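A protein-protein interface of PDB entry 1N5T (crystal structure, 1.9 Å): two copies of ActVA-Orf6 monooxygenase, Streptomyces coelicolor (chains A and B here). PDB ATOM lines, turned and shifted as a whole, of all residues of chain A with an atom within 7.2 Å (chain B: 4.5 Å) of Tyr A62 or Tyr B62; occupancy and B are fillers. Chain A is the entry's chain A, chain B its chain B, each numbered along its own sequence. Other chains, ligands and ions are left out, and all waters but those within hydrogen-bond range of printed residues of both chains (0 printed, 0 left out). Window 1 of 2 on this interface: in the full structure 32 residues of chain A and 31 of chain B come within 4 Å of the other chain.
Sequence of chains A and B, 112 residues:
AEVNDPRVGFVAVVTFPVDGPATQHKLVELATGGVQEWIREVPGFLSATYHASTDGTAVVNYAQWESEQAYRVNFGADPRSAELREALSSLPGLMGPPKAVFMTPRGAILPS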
ATOM      1  N   ALA A   1     -21.861  22.618 -12.195  1.00  0.00           N
ATOM      2  CA  ALA A   1     -22.389  22.218 -13.525  1.00  0.00           C
ATOM      3  C   ALA A   1     -23.195  23.375 -14.115  1.00  0.00           C
ATOM      4  O   ALA A   1     -23.549  24.289 -13.367  1.00  0.00           O
ATOM      5  CB  ALA A   1     -23.267  21.003 -13.397  1.00  0.00           C
ATOM      6  N   GLU A   2     -23.431  23.334 -15.421  1.00  0.00           N
ATOM      7  CA  GLU A   2     -24.290  24.345 -16.050  1.00  0.00           C
ATOM      8  C   GLU A   2     -25.527  24.431 -15.158  1.00  0.00           C
ATOM      9  O   GLU A   2     -25.899  23.400 -14.584  1.00  0.00           O
ATOM     10  CB  GLU A   2     -24.665  23.921 -17.467  1.00  0.00           C
ATOM     11  CG  GLU A   2     -23.454  23.486 -18.308  1.00  0.00           C
ATOM     12  CD  GLU A   2     -22.536  24.610 -18.689  1.00  0.00           C
ATOM     13  OE1 GLU A   2     -22.452  25.570 -17.880  1.00  0.00           O
ATOM     14  OE2 GLU A   2     -21.867  24.612 -19.760  1.00  0.00           O
ATOM     15  N   VAL A   3     -26.119  25.611 -14.987  1.00  0.00           N
ATOM     16  CA  VAL A   3     -27.246  25.730 -14.053  1.00  0.00           C
ATOM     17  C   VAL A   3     -28.483  24.948 -14.442  1.00  0.00           C
ATOM     18  O   VAL A   3     -29.397  24.747 -13.631  1.00  0.00           O
ATOM     19  CB  VAL A   3     -27.614  27.244 -13.911  1.00  0.00           C
ATOM     20  CG1 VAL A   3     -26.489  27.892 -13.099  1.00  0.00           C
ATOM     21  CG2 VAL A   3     -27.791  27.936 -15.250  1.00  0.00           C
ATOM     22  N   ASN A   4     -28.570  24.601 -15.726  1.00  0.00           N
ATOM     23  CA  ASN A   4     -29.721  23.886 -16.248  1.00  0.00           C
ATOM     24  C   ASN A   4     -29.382  22.451 -16.616  1.00  0.00           C
ATOM     25  O   ASN A   4     -30.241  21.763 -17.181  1.00  0.00           O
ATOM     26  CB  ASN A   4     -30.352  24.632 -17.436  1.00  0.00           C
ATOM     27  CG  ASN A   4     -29.434  24.713 -18.636  1.00  0.00           C
ATOM     28  OD1 ASN A   4     -28.218  24.823 -18.495  1.00  0.00           O
ATOM     29  ND2 ASN A   4     -30.038  24.671 -19.832  1.00  0.00           N
ATOM     30  N   VAL A   8     -28.619  17.996 -12.476  1.00  0.00           N
ATOM     31  CA  VAL A   8     -28.891  18.645 -11.187  1.00  0.00           C
ATOM     32  C   VAL A   8     -30.299  18.285 -10.688  1.00  0.00           C
ATOM     33  O   VAL A   8     -31.303  18.797 -11.191  1.00  0.00           O
ATOM     34  CB  VAL A   8     -28.713  20.169 -11.240  1.00  0.00           C
ATOM     35  CG1 VAL A   8     -28.982  20.751  -9.842  1.00  0.00           C
ATOM     36  CG2 VAL A   8     -27.308  20.481 -11.707  1.00  0.00           C
ATOM     37  N   PHE A  10     -30.974  18.233  -7.150  1.00  0.00           N
ATOM     38  CA  PHE A  10     -31.284  18.707  -5.811  1.00  0.00           C
ATOM     39  C   PHE A  10     -30.371  19.900  -5.499  1.00  0.00           C
ATOM     40  O   PHE A  10     -29.223  19.873  -5.907  1.00  0.00           O
ATOM     41  CB  PHE A  10     -31.120  17.588  -4.770  1.00  0.00           C
ATOM     42  CG  PHE A  10     -31.462  17.934  -3.361  1.00  0.00           C
ATOM     43  CD1 PHE A  10     -32.800  17.879  -2.960  1.00  0.00           C
ATOM     44  CD2 PHE A  10     -30.505  18.338  -2.452  1.00  0.00           C
ATOM     45  CE1 PHE A  10     -33.177  18.201  -1.670  1.00  0.00           C
ATOM     46  CE2 PHE A  10     -30.889  18.640  -1.143  1.00  0.00           C
ATOM     47  CZ  PHE A  10     -32.193  18.579  -0.770  1.00  0.00           C
ATOM     48  N   VAL A  11     -31.004  20.923  -4.929  1.00  0.00           N
ATOM     49  CA  VAL A  11     -30.255  22.169  -4.661  1.00  0.00           C
ATOM     50  C   VAL A  11     -30.544  22.597  -3.232  1.00  0.00           C
ATOM     51  O   VAL A  11     -31.645  22.584  -2.689  1.00  0.00           O
ATOM     52  CB  VAL A  11     -30.639  23.287  -5.625  1.00  0.00           C
ATOM     53  CG1 VAL A  11     -30.124  24.720  -5.152  1.00  0.00           C
ATOM     54  CG2 VAL A  11     -30.184  23.064  -7.065  1.00  0.00           C
ATOM     55  N   ALA A  12     -29.500  23.073  -2.554  1.00  0.00           N
ATOM     56  CA  ALA A  12     -29.533  23.653  -1.238  1.00  0.00           C
ATOM     57  C   ALA A  12     -28.948  25.084  -1.366  1.00  0.00           C
ATOM     58  O   ALA A  12     -27.885  25.267  -1.970  1.00  0.00           O
ATOM     59  CB  ALA A  12     -28.633  22.889  -0.245  1.00  0.00           C
ATOM     60  N   VAL A  13     -29.682  26.058  -0.876  1.00  0.00           N
ATOM     61  CA  VAL A  13     -29.256  27.478  -0.857  1.00  0.00           C
ATOM     62  C   VAL A  13     -29.155  27.776   0.637  1.00  0.00           C
ATOM     63  O   VAL A  13     -30.149  27.718   1.387  1.00  0.00           O
ATOM     64  CB  VAL A  13     -30.207  28.446  -1.532  1.00  0.00           C
ATOM     65  CG1 VAL A  13     -29.724  29.888  -1.388  1.00  0.00           C
ATOM     66  CG2 VAL A  13     -30.352  28.027  -2.999  1.00  0.00           C
ATOM     67  N   VAL A  14     -27.878  27.988   1.036  1.00  0.00           N
ATOM     68  CA  VAL A  14     -27.536  28.152   2.423  1.00  0.00           C
ATOM     69  C   VAL A  14     -26.976  29.567   2.688  1.00  0.00           C
ATOM     70  O   VAL A  14     -26.019  30.006   2.058  1.00  0.00           O
ATOM     71  CB  VAL A  14     -26.473  27.085   2.837  1.00  0.00           C
ATOM     72  CG1 VAL A  14     -26.200  27.251   4.304  1.00  0.00           C
ATOM     73  CG2 VAL A  14     -26.962  25.659   2.479  1.00  0.00           C
ATOM     74  N   SER A  47     -21.502  20.935  -7.205  1.00  0.00           N
ATOM     75  CA  SER A  47     -20.776  22.204  -6.978  1.00  0.00           C
ATOM     76  C   SER A  47     -21.286  22.907  -5.725  1.00  0.00           C
ATOM     77  O   SER A  47     -22.382  22.603  -5.212  1.00  0.00           O
ATOM     78  CB  SER A  47     -21.058  23.159  -8.147  1.00  0.00           C
ATOM     79  OG  SER A  47     -22.377  23.701  -8.138  1.00  0.00           O
ATOM     80  N   ALA A  48     -20.436  23.806  -5.210  1.00  0.00           N
ATOM     81  CA  ALA A  48     -20.866  24.694  -4.126  1.00  0.00           C
ATOM     82  C   ALA A  48     -20.323  26.091  -4.451  1.00  0.00           C
ATOM     83  O   ALA A  48     -19.093  26.189  -4.496  1.00  0.00           O
ATOM     84  CB  ALA A  48     -20.383  24.194  -2.803  1.00  0.00           C
ATOM     85  N   THR A  49     -21.184  27.058  -4.748  1.00  0.00           N
ATOM     86  CA  THR A  49     -20.706  28.380  -5.090  1.00  0.00           C
ATOM     87  C   THR A  49     -20.980  29.378  -3.996  1.00  0.00           C
ATOM     88  O   THR A  49     -22.139  29.476  -3.587  1.00  0.00           O
ATOM     89  CB  THR A  49     -21.320  28.849  -6.431  1.00  0.00           C
ATOM     90  OG1 THR A  49     -20.820  27.907  -7.418  1.00  0.00           O
ATOM     91  CG2 THR A  49     -20.793  30.258  -6.726  1.00  0.00           C
ATOM     92  N   TYR A  50     -19.935  29.980  -3.441  1.00  0.00           N
ATOM     93  CA  TYR A  50     -20.140  30.900  -2.307  1.00  0.00           C
ATOM     94  C   TYR A  50     -20.157  32.320  -2.843  1.00  0.00           C
ATOM     95  O   TYR A  50     -19.228  32.710  -3.586  1.00  0.00           O
ATOM     96  CB  TYR A  50     -19.049  30.739  -1.238  1.00  0.00           C
ATOM     97  CG  TYR A  50     -19.187  29.436  -0.456  1.00  0.00           C
ATOM     98  CD1 TYR A  50     -18.831  28.221  -1.034  1.00  0.00           C
ATOM     99  CD2 TYR A  50     -19.746  29.454   0.805  1.00  0.00           C
ATOM    100  CE1 TYR A  50     -19.066  27.046  -0.340  1.00  0.00           C
ATOM    101  CE2 TYR A  50     -19.962  28.280   1.501  1.00  0.00           C
ATOM    102  CZ  TYR A  50     -19.577  27.091   0.919  1.00  0.00           C
ATOM    103  OH  TYR A  50     -19.771  25.936   1.640  1.00  0.00           O
ATOM    104  N   HIS A  51     -21.184  33.085  -2.433  1.00  0.00           N
ATOM    105  CA  HIS A  51     -21.303  34.447  -2.882  1.00  0.00           C
ATOM    106  C   HIS A  51     -21.285  35.447  -1.711  1.00  0.00           C
ATOM    107  O   HIS A  51     -21.810  35.047  -0.655  1.00  0.00           O
ATOM    108  CB  HIS A  51     -22.696  34.605  -3.547  1.00  0.00           C
ATOM    109  CG  HIS A  51     -23.044  33.621  -4.624  1.00  0.00           C
ATOM    110  ND1 HIS A  51     -23.367  32.333  -4.314  1.00  0.00           N
ATOM    111  CD2 HIS A  51     -23.188  33.735  -5.962  1.00  0.00           C
ATOM    112  CE1 HIS A  51     -23.695  31.637  -5.421  1.00  0.00           C
ATOM    113  NE2 HIS A  51     -23.622  32.509  -6.453  1.00  0.00           N
ATOM    114  N   VAL A  60     -23.797  33.518   0.803  1.00  0.00           N
ATOM    115  CA  VAL A  60     -24.838  32.531   0.400  1.00  0.00           C
ATOM    116  C   VAL A  60     -24.133  31.469  -0.431  1.00  0.00           C
ATOM    117  O   VAL A  60     -23.434  31.793  -1.446  1.00  0.00           O
ATOM    118  CB  VAL A  60     -25.794  33.246  -0.573  1.00  0.00           C
ATOM    119  CG1 VAL A  60     -26.743  32.207  -1.175  1.00  0.00           C
ATOM    120  CG2 VAL A  60     -26.577  34.292   0.225  1.00  0.00           C
ATOM    121  N   ASN A  61     -24.461  30.220  -0.121  1.00  0.00           N
ATOM    122  CA  ASN A  61     -23.915  29.085  -0.896  1.00  0.00           C
ATOM    123  C   ASN A  61     -25.077  28.454  -1.730  1.00  0.00           C
ATOM    124  O   ASN A  61     -26.104  28.155  -1.144  1.00  0.00           O
ATOM    125  CB  ASN A  61     -23.415  28.024   0.077  1.00  0.00           C
ATOM    126  CG  ASN A  61     -23.065  26.656  -0.466  1.00  0.00           C
ATOM    127  OD1 ASN A  61     -22.762  26.487  -1.633  1.00  0.00           O
ATOM    128  ND2 ASN A  61     -23.030  25.620   0.400  1.00  0.00           N
ATOM    129  N   TYR A  62     -24.954  28.392  -3.027  1.00  0.00           N
ATOM    130  CA  TYR A  62     -25.834  27.736  -3.994  1.00  0.00           C
ATOM    131  C   TYR A  62     -25.151  26.405  -4.312  1.00  0.00           C
ATOM    132  O   TYR A  62     -24.056  26.404  -4.918  1.00  0.00           O
ATOM    133  CB  TYR A  62     -25.969  28.607  -5.257  1.00  0.00           C
ATOM    134  CG  TYR A  62     -26.857  27.999  -6.327  1.00  0.00           C
ATOM    135  CD1 TYR A  62     -28.219  28.103  -6.229  1.00  0.00           C
ATOM    136  CD2 TYR A  62     -26.296  27.296  -7.402  1.00  0.00           C
ATOM    137  CE1 TYR A  62     -29.091  27.482  -7.172  1.00  0.00           C
ATOM    138  CE2 TYR A  62     -27.147  26.663  -8.352  1.00  0.00           C
ATOM    139  CZ  TYR A  62     -28.515  26.793  -8.212  1.00  0.00           C
ATOM    140  OH  TYR A  62     -29.327  26.166  -9.134  1.00  0.00           O
ATOM    141  N   ALA A  63     -25.684  25.301  -3.801  1.00  0.00           N
ATOM    142  CA  ALA A  63     -25.055  23.983  -3.970  1.00  0.00           C
ATOM    143  C   ALA A  63     -25.901  23.050  -4.838  1.00  0.00           C
ATOM    144  O   ALA A  63     -27.087  22.967  -4.565  1.00  0.00           O
ATOM    145  CB  ALA A  63     -24.790  23.345  -2.639  1.00  0.00           C
ATOM    146  N   GLN A  64     -25.291  22.429  -5.822  1.00  0.00           N
ATOM    147  CA  GLN A  64     -25.936  21.556  -6.784  1.00  0.00           C
ATOM    148  C   GLN A  64     -25.526  20.112  -6.450  1.00  0.00           C
ATOM    149  O   GLN A  64     -24.358  19.817  -6.175  1.00  0.00           O
ATOM    150  CB  GLN A  64     -25.379  21.841  -8.197  1.00  0.00           C
ATOM    151  CG  GLN A  64     -25.708  23.191  -8.796  1.00  0.00           C
ATOM    152  CD  GLN A  64     -24.977  23.366 -10.142  1.00  0.00           C
ATOM    153  OE1 GLN A  64     -23.771  23.112 -10.224  1.00  0.00           O
ATOM    154  NE2 GLN A  64     -25.653  23.799 -11.178  1.00  0.00           N
ATOM    155  N   MET A 103     -34.557  22.647  -2.495  1.00  0.00           N
ATOM    156  CA  MET A 103     -35.350  22.833  -3.701  1.00  0.00           C
ATOM    157  C   MET A 103     -34.830  22.002  -4.858  1.00  0.00           C
ATOM    158  O   MET A 103     -33.746  21.390  -4.905  1.00  0.00           O
ATOM    159  CB  MET A 103     -35.260  24.351  -4.063  1.00  0.00           C
ATOM    160  CG  MET A 103     -33.889  24.815  -4.503  1.00  0.00           C
ATOM    161  SD  MET A 103     -33.672  26.625  -4.599  1.00  0.00           S
ATOM    162  CE  MET A 103     -33.867  27.084  -2.902  1.00  0.00           C
ATOM    163  N   PRO A 105     -34.691  22.135  -9.198  1.00  0.00           N
ATOM    164  CA  PRO A 105     -34.762  22.961 -10.389  1.00  0.00           C
ATOM    165  C   PRO A 105     -35.983  22.555 -11.231  1.00  0.00           C
ATOM    166  O   PRO A 105     -36.273  21.356 -11.290  1.00  0.00           O
ATOM    167  CB  PRO A 105     -33.462  22.770 -11.101  1.00  0.00           C
ATOM    168  CG  PRO A 105     -32.628  21.839 -10.292  1.00  0.00           C
ATOM    169  CD  PRO A 105     -33.493  21.266  -9.192  1.00  0.00           C
ATOM    170  N   VAL B  11     -25.229  38.192  -9.316  1.00  0.00           N
ATOM    171  CA  VAL B  11     -26.284  37.191  -9.189  1.00  0.00           C
ATOM    172  C   VAL B  11     -27.477  37.728  -8.406  1.00  0.00           C
ATOM    173  O   VAL B  11     -27.245  38.394  -7.402  1.00  0.00           O
ATOM    174  CB  VAL B  11     -25.724  35.940  -8.399  1.00  0.00           C
ATOM    175  CG1 VAL B  11     -26.888  35.017  -7.972  1.00  0.00           C
ATOM    176  CG2 VAL B  11     -24.745  35.177  -9.323  1.00  0.00           C
ATOM    177  N   ALA B  12     -28.687  37.360  -8.840  1.00  0.00           N
ATOM    178  CA  ALA B  12     -29.839  37.708  -7.984  1.00  0.00           C
ATOM    179  C   ALA B  12     -30.511  36.373  -7.616  1.00  0.00           C
ATOM    180  O   ALA B  12     -30.584  35.436  -8.454  1.00  0.00           O
ATOM    181  CB  ALA B  12     -30.802  38.599  -8.768  1.00  0.00           C
ATOM    182  N   VAL B  13     -30.996  36.233  -6.409  1.00  0.00           N
ATOM    183  CA  VAL B  13     -31.681  35.045  -5.907  1.00  0.00           C
ATOM    184  C   VAL B  13     -33.018  35.652  -5.410  1.00  0.00           C
ATOM    185  O   VAL B  13     -33.036  36.422  -4.451  1.00  0.00           O
ATOM    186  CB  VAL B  13     -30.956  34.323  -4.787  1.00  0.00           C
ATOM    187  CG1 VAL B  13     -31.758  33.166  -4.192  1.00  0.00           C
ATOM    188  CG2 VAL B  13     -29.588  33.742  -5.278  1.00  0.00           C
ATOM    189  N   SER B  47     -28.339  33.765 -17.264  1.00  0.00           N
ATOM    190  CA  SER B  47     -29.301  32.697 -17.053  1.00  0.00           C
ATOM    191  C   SER B  47     -30.305  33.018 -15.962  1.00  0.00           C
ATOM    192  O   SER B  47     -29.993  33.927 -15.191  1.00  0.00           O
ATOM    193  CB  SER B  47     -28.681  31.365 -16.576  1.00  0.00           C
ATOM    194  OG  SER B  47     -28.121  31.616 -15.244  1.00  0.00           O
ATOM    195  N   ALA B  48     -31.443  32.323 -16.023  1.00  0.00           N
ATOM    196  CA  ALA B  48     -32.383  32.383 -14.892  1.00  0.00           C
ATOM    197  C   ALA B  48     -32.899  30.958 -14.666  1.00  0.00           C
ATOM    198  O   ALA B  48     -33.436  30.296 -15.585  1.00  0.00           O
ATOM    199  CB  ALA B  48     -33.467  33.404 -15.105  1.00  0.00           C
ATOM    200  N   THR B  49     -32.636  30.333 -13.525  1.00  0.00           N
ATOM    201  CA  THR B  49     -33.055  28.973 -13.200  1.00  0.00           C
ATOM    202  C   THR B  49     -34.064  28.984 -12.057  1.00  0.00           C
ATOM    203  O   THR B  49     -33.746  29.389 -10.914  1.00  0.00           O
ATOM    204  CB  THR B  49     -31.853  28.108 -12.791  1.00  0.00           C
ATOM    205  OG1 THR B  49     -30.900  28.234 -13.836  1.00  0.00           O
ATOM    206  CG2 THR B  49     -32.225  26.643 -12.560  1.00  0.00           C
ATOM    207  N   HIS B  51     -36.616  27.197  -9.444  1.00  0.00           N
ATOM    208  CA  HIS B  51     -36.672  25.990  -8.633  1.00  0.00           C
ATOM    209  C   HIS B  51     -37.937  25.955  -7.815  1.00  0.00           C
ATOM    210  O   HIS B  51     -38.396  27.031  -7.483  1.00  0.00           O
ATOM    211  CB  HIS B  51     -35.530  25.963  -7.565  1.00  0.00           C
ATOM    212  CG  HIS B  51     -34.156  26.211  -8.128  1.00  0.00           C
ATOM    213  ND1 HIS B  51     -33.807  27.469  -8.569  1.00  0.00           N
ATOM    214  CD2 HIS B  51     -33.040  25.438  -8.236  1.00  0.00           C
ATOM    215  CE1 HIS B  51     -32.523  27.468  -8.992  1.00  0.00           C
ATOM    216  NE2 HIS B  51     -32.065  26.248  -8.765  1.00  0.00           N
ATOM    217  N   VAL B  60     -37.914  29.790  -6.298  1.00  0.00           N
ATOM    218  CA  VAL B  60     -36.675  30.586  -6.159  1.00  0.00           C
ATOM    219  C   VAL B  60     -35.990  30.594  -7.546  1.00  0.00           C
ATOM    220  O   VAL B  60     -35.783  29.551  -8.203  1.00  0.00           O
ATOM    221  CB  VAL B  60     -35.674  29.914  -5.190  1.00  0.00           C
ATOM    222  CG1 VAL B  60     -34.382  30.753  -5.094  1.00  0.00           C
ATOM    223  CG2 VAL B  60     -36.231  29.751  -3.800  1.00  0.00           C
ATOM    224  N   ASN B  61     -35.626  31.805  -7.952  1.00  0.00           N
ATOM    225  CA  ASN B  61     -34.913  31.981  -9.198  1.00  0.00           C
ATOM    226  C   ASN B  61     -33.456  32.322  -8.849  1.00  0.00           C
ATOM    227  O   ASN B  61     -33.218  33.317  -8.149  1.00  0.00           O
ATOM    228  CB  ASN B  61     -35.573  33.141  -9.973  1.00  0.00           C
ATOM    229  CG  ASN B  61     -34.820  33.645 -11.186  1.00  0.00           C
ATOM    230  OD1 ASN B  61     -33.941  32.973 -11.700  1.00  0.00           O
ATOM    231  ND2 ASN B  61     -35.129  34.846 -11.706  1.00  0.00           N
ATOM    232  N   TYR B  62     -32.530  31.560  -9.362  1.00  0.00           N
ATOM    233  CA  TYR B  62     -31.081  31.870  -9.203  1.00  0.00           C
ATOM    234  C   TYR B  62     -30.707  32.457 -10.587  1.00  0.00           C
ATOM    235  O   TYR B  62     -30.803  31.715 -11.573  1.00  0.00           O
ATOM    236  CB  TYR B  62     -30.278  30.617  -8.913  1.00  0.00           C
ATOM    237  CG  TYR B  62     -28.759  30.842  -8.840  1.00  0.00           C
ATOM    238  CD1 TYR B  62     -27.979  30.600  -9.987  1.00  0.00           C
ATOM    239  CD2 TYR B  62     -28.171  31.262  -7.691  1.00  0.00           C
ATOM    240  CE1 TYR B  62     -26.604  30.799  -9.964  1.00  0.00           C
ATOM    241  CE2 TYR B  62     -26.763  31.472  -7.638  1.00  0.00           C
ATOM    242  CZ  TYR B  62     -26.039  31.231  -8.765  1.00  0.00           C
ATOM    243  OH  TYR B  62     -24.657  31.385  -8.727  1.00  0.00           O
ATOM    244  N   ALA B  63     -30.371  33.742 -10.684  1.00  0.00           N
ATOM    245  CA  ALA B  63     -30.176  34.367 -12.009  1.00  0.00           C
ATOM    246  C   ALA B  63     -28.739  34.887 -12.174  1.00  0.00           C
ATOM    247  O   ALA B  63     -28.245  35.563 -11.268  1.00  0.00           O
ATOM    248  CB  ALA B  63     -31.188  35.536 -12.118  1.00  0.00           C
ATOM    249  N   GLN B  64     -28.098  34.601 -13.285  1.00  0.00           N
ATOM    250  CA  GLN B  64     -26.704  34.993 -13.496  1.00  0.00           C
ATOM    251  C   GLN B  64     -26.616  36.157 -14.505  1.00  0.00           C
ATOM    252  O   GLN B  64     -27.362  36.090 -15.505  1.00  0.00           O
ATOM    253  CB  GLN B  64     -25.923  33.834 -14.103  1.00  0.00           C
ATOM    254  CG  GLN B  64     -25.783  32.604 -13.176  1.00  0.00           C
ATOM    255  CD  GLN B  64     -25.156  31.484 -13.995  1.00  0.00           C
ATOM    256  OE1 GLN B  64     -25.614  31.190 -15.113  1.00  0.00           O
ATOM    257  NE2 GLN B  64     -24.147  30.848 -13.432  1.00  0.00           N
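The side-chain hydroxyl (OH) of Tyr B62 is in hydrogen-bond range of a ring nitrogen (NE2) of His A51. The side-chain hydroxyl of Tyr A62 lies within hydrogen-bond range of a ring nitrogen (NE2) of His B51, at 2.8 Å.
Printed residues of chain B within 4 Å of Val A3: Ser B47, Thr B49 and Gln B64. Tyr A50 touches none of the printed residues of chain B. Of chain B, only His B51 (2.8 Å) and Tyr B62 (3.5 Å) come within 4 Å of Tyr A62. Of the printed residues of chain B, Pro A105 touches His B51 (3.7 Å). Ala B12 touches none of the printed residues of chain A. Of the printed residues of chain A, Ser B47 touches Val A3. Printed residues of chain A within 4 Å of Thr B49: Val A3. Printed residues of chain A within 4 Å of Gln B64: Val A3 (3.8 Å). The nearest printed residue of chain B that does not touch Met A103 is Asn B61 (6.5 Å).
CG2 of Val A3 touches OG of Ser B47 (3.7 Å). OG1 of Thr B49 touches CG2 of Val A3, 3.4 Å away. Val A3 touches Gln B64 (CG1 to NE2, 3.8 Å). Val A11 touches His B51. Val B11 touches His A51. Tyr A62 touches Tyr B62 (CD1 to CD2, 3.5 Å). Met A103 touches His B51. CE of Met A103 touches CG2 of Val B60, 3.7 Å away. Pro A105 touches His B51 (CA to CD2, 3.7 Å).
The backbone NH (N) of Thr A49 sits at hydrogen-bond distance from the backbone carbonyl oxygen (O) of Tyr A62 (3.0 Å). The side-chain amide oxygen (OE1) of Gln B64 sits at hydrogen-bond distance from the side-chain hydroxyl (OG) of Ser B47, at 2.5 Å. O of Thr B49 lies close to ND1 of His B51 (3.0 Å). The side-chain amide oxygen of Asn B61 sits at hydrogen-bond distance from the backbone NH of Thr B49, at 3.5 Å. N of Tyr B62 sits at hydrogen-bond distance from O of Thr B49, 2.9 Å away. The backbone NH (N) of His B51 is in hydrogen-bond range of the backbone carbonyl oxygen (O) of Val B60 (2.8 Å).
Of the 12 printed residues of chain B, 7 touch a printed residue of chain A. Printed residues of chain B that touch a printed residue of chain A: Val B11, Ser B47, Thr B49, His B51, Val B60, Tyr B62 and Gln B64. Printed residues of chain A that touch a printed residue of chain B: Val A3, Val A11, His A51, Tyr A62, Met A103 and Pro A105. Hydrophobic or aromatic side chains of chain A within 4 Å of the printed part of chain B: Val A3, Val A11, His A51, Tyr A62, Met A103 and Pro A105.
Val A11 touches His B51, and with the chains exchanged His A51 touches Val B11. His A51 touches Tyr B62, and with the chains exchanged Tyr A62 touches His B51. Tyr B62 touches its own counterpart, Tyr A62.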
